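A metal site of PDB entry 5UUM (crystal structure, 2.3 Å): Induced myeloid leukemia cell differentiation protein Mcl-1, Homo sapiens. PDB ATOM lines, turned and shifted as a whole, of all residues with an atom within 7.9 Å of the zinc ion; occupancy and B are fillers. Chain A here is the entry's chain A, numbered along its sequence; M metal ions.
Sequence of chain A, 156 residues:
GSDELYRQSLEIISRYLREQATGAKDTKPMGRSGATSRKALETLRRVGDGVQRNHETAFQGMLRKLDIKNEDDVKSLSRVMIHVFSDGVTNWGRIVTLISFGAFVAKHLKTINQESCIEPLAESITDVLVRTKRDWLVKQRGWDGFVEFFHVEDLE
The zinc ion is bound by the side-chain carboxylate of Glu 153, a ring nitrogen (ND1) of His 151 and the side-chain carboxylate of Glu 148.
Three residues have an atom within 4 Å of the zinc ion: Glu 148, His 151 and Glu 153.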
ATOM      1  N   LYS A  39     -18.757 -21.225   1.643  1.00  0.00           N
ATOM      2  CA  LYS A  39     -19.343 -19.960   1.222  1.00  0.00           C
ATOM      3  C   LYS A  39     -19.364 -18.944   2.355  1.00  0.00           C
ATOM      4  O   LYS A  39     -19.232 -17.735   2.103  1.00  0.00           O
ATOM      5  CB  LYS A  39     -20.753 -20.205   0.680  1.00  0.00           C
ATOM      6  CG  LYS A  39     -20.790 -21.126  -0.541  1.00  0.00           C
ATOM      7  CD  LYS A  39     -22.201 -21.513  -0.935  1.00  0.00           C
ATOM      8  CE  LYS A  39     -22.959 -20.361  -1.554  1.00  0.00           C
ATOM      9  NZ  LYS A  39     -24.303 -20.779  -2.033  1.00  0.00           N
ATOM     10  N   ASP A 144     -26.054 -20.353   6.700  1.00  0.00           N
ATOM     11  CA  ASP A 144     -26.763 -20.156   5.438  1.00  0.00           C
ATOM     12  C   ASP A 144     -27.439 -18.788   5.406  1.00  0.00           C
ATOM     13  O   ASP A 144     -27.445 -18.107   4.373  1.00  0.00           O
ATOM     14  CB  ASP A 144     -27.779 -21.269   5.208  1.00  0.00           C
ATOM     15  CG  ASP A 144     -27.122 -22.624   4.977  1.00  0.00           C
ATOM     16  OD1 ASP A 144     -26.153 -22.699   4.197  1.00  0.00           O
ATOM     17  OD2 ASP A 144     -27.585 -23.619   5.592  1.00  0.00           O
ATOM     18  N   VAL A 147     -24.640 -16.154   4.976  1.00  0.00           N
ATOM     19  CA  VAL A 147     -24.214 -16.063   3.579  1.00  0.00           C
ATOM     20  C   VAL A 147     -25.212 -15.226   2.786  1.00  0.00           C
ATOM     21  O   VAL A 147     -24.828 -14.295   2.061  1.00  0.00           O
ATOM     22  CB  VAL A 147     -24.047 -17.473   2.980  1.00  0.00           C
ATOM     23  CG1 VAL A 147     -23.937 -17.413   1.459  1.00  0.00           C
ATOM     24  CG2 VAL A 147     -22.820 -18.146   3.569  1.00  0.00           C
ATOM     25  N   GLU A 148     -26.501 -15.562   2.890  1.00  0.00           N
ATOM     26  CA  GLU A 148     -27.506 -14.927   2.039  1.00  0.00           C
ATOM     27  C   GLU A 148     -27.682 -13.455   2.381  1.00  0.00           C
ATOM     28  O   GLU A 148     -27.807 -12.611   1.491  1.00  0.00           O
ATOM     29  CB  GLU A 148     -28.837 -15.677   2.160  1.00  0.00           C
ATOM     30  CG  GLU A 148     -28.805 -17.076   1.559  1.00  0.00           C
ATOM     31  CD  GLU A 148     -28.426 -17.063   0.089  1.00  0.00           C
ATOM     32  OE1 GLU A 148     -28.900 -16.161  -0.638  1.00  0.00           O
ATOM     33  OE2 GLU A 148     -27.641 -17.943  -0.338  1.00  0.00           O
ATOM     34  N   PHE A 149     -27.678 -13.114   3.677  1.00  0.00           N
ATOM     35  CA  PHE A 149     -27.850 -11.721   4.068  1.00  0.00           C
ATOM     36  C   PHE A 149     -26.846 -10.821   3.359  1.00  0.00           C
ATOM     37  O   PHE A 149     -27.194  -9.727   2.892  1.00  0.00           O
ATOM     38  CB  PHE A 149     -27.704 -11.589   5.586  1.00  0.00           C
ATOM     39  CG  PHE A 149     -27.736 -10.174   6.073  1.00  0.00           C
ATOM     40  CD1 PHE A 149     -28.938  -9.559   6.376  1.00  0.00           C
ATOM     41  CD2 PHE A 149     -26.563  -9.452   6.237  1.00  0.00           C
ATOM     42  CE1 PHE A 149     -28.972  -8.256   6.819  1.00  0.00           C
ATOM     43  CE2 PHE A 149     -26.589  -8.152   6.686  1.00  0.00           C
ATOM     44  CZ  PHE A 149     -27.793  -7.556   6.983  1.00  0.00           C
ATOM     45  N   PHE A 150     -25.590 -11.264   3.264  1.00  0.00           N
ATOM     46  CA  PHE A 150     -24.527 -10.484   2.651  1.00  0.00           C
ATOM     47  C   PHE A 150     -24.326 -10.812   1.171  1.00  0.00           C
ATOM     48  O   PHE A 150     -23.343 -10.359   0.579  1.00  0.00           O
ATOM     49  CB  PHE A 150     -23.213 -10.700   3.403  1.00  0.00           C
ATOM     50  CG  PHE A 150     -23.204 -10.112   4.781  1.00  0.00           C
ATOM     51  CD1 PHE A 150     -23.225  -8.736   4.961  1.00  0.00           C
ATOM     52  CD2 PHE A 150     -23.169 -10.930   5.907  1.00  0.00           C
ATOM     53  CE1 PHE A 150     -23.210  -8.187   6.228  1.00  0.00           C
ATOM     54  CE2 PHE A 150     -23.154 -10.381   7.173  1.00  0.00           C
ATOM     55  CZ  PHE A 150     -23.178  -9.010   7.338  1.00  0.00           C
ATOM     56  N   HIS A 151     -25.214 -11.592   0.565  1.00  0.00           N
ATOM     57  CA  HIS A 151     -25.090 -11.973  -0.834  1.00  0.00           C
ATOM     58  C   HIS A 151     -25.878 -11.003  -1.696  1.00  0.00           C
ATOM     59  O   HIS A 151     -27.106 -10.897  -1.573  1.00  0.00           O
ATOM     60  CB  HIS A 151     -25.582 -13.402  -1.056  1.00  0.00           C
ATOM     61  CG  HIS A 151     -25.420 -13.887  -2.464  1.00  0.00           C
ATOM     62  ND1 HIS A 151     -26.369 -14.652  -3.103  1.00  0.00           N
ATOM     63  CD2 HIS A 151     -24.429 -13.693  -3.367  1.00  0.00           C
ATOM     64  CE1 HIS A 151     -25.970 -14.931  -4.327  1.00  0.00           C
ATOM     65  NE2 HIS A 151     -24.789 -14.350  -4.510  1.00  0.00           N
ATOM     66  N   VAL A 152     -25.182 -10.303  -2.593  1.00  0.00           N
ATOM     67  CA  VAL A 152     -25.816  -9.385  -3.528  1.00  0.00           C
ATOM     68  C   VAL A 152     -26.389 -10.194  -4.674  1.00  0.00           C
ATOM     69  O   VAL A 152     -25.653 -10.899  -5.374  1.00  0.00           O
ATOM     70  CB  VAL A 152     -24.829  -8.330  -4.026  1.00  0.00           C
ATOM     71  CG1 VAL A 152     -25.549  -7.257  -4.832  1.00  0.00           C
ATOM     72  CG2 VAL A 152     -24.075  -7.710  -2.858  1.00  0.00           C
ATOM     73  N   GLU A 153     -27.703 -10.089  -4.886  1.00  0.00           N
ATOM     74  CA  GLU A 153     -28.393 -10.969  -5.818  1.00  0.00           C
ATOM     75  C   GLU A 153     -28.487 -10.402  -7.230  1.00  0.00           C
ATOM     76  O   GLU A 153     -28.613 -11.180  -8.185  1.00  0.00           O
ATOM     77  CB  GLU A 153     -29.793 -11.284  -5.297  1.00  0.00           C
ATOM     78  CG  GLU A 153     -29.796 -12.106  -4.018  1.00  0.00           C
ATOM     79  CD  GLU A 153     -29.318 -13.524  -4.242  1.00  0.00           C
ATOM     80  OE1 GLU A 153     -29.036 -13.875  -5.410  1.00  0.00           O
ATOM     81  OE2 GLU A 153     -29.236 -14.289  -3.261  1.00  0.00           O
HETATM   82 ZN    ZN M   1     -28.149 -15.531  -2.605  1.00  0.00          ZN
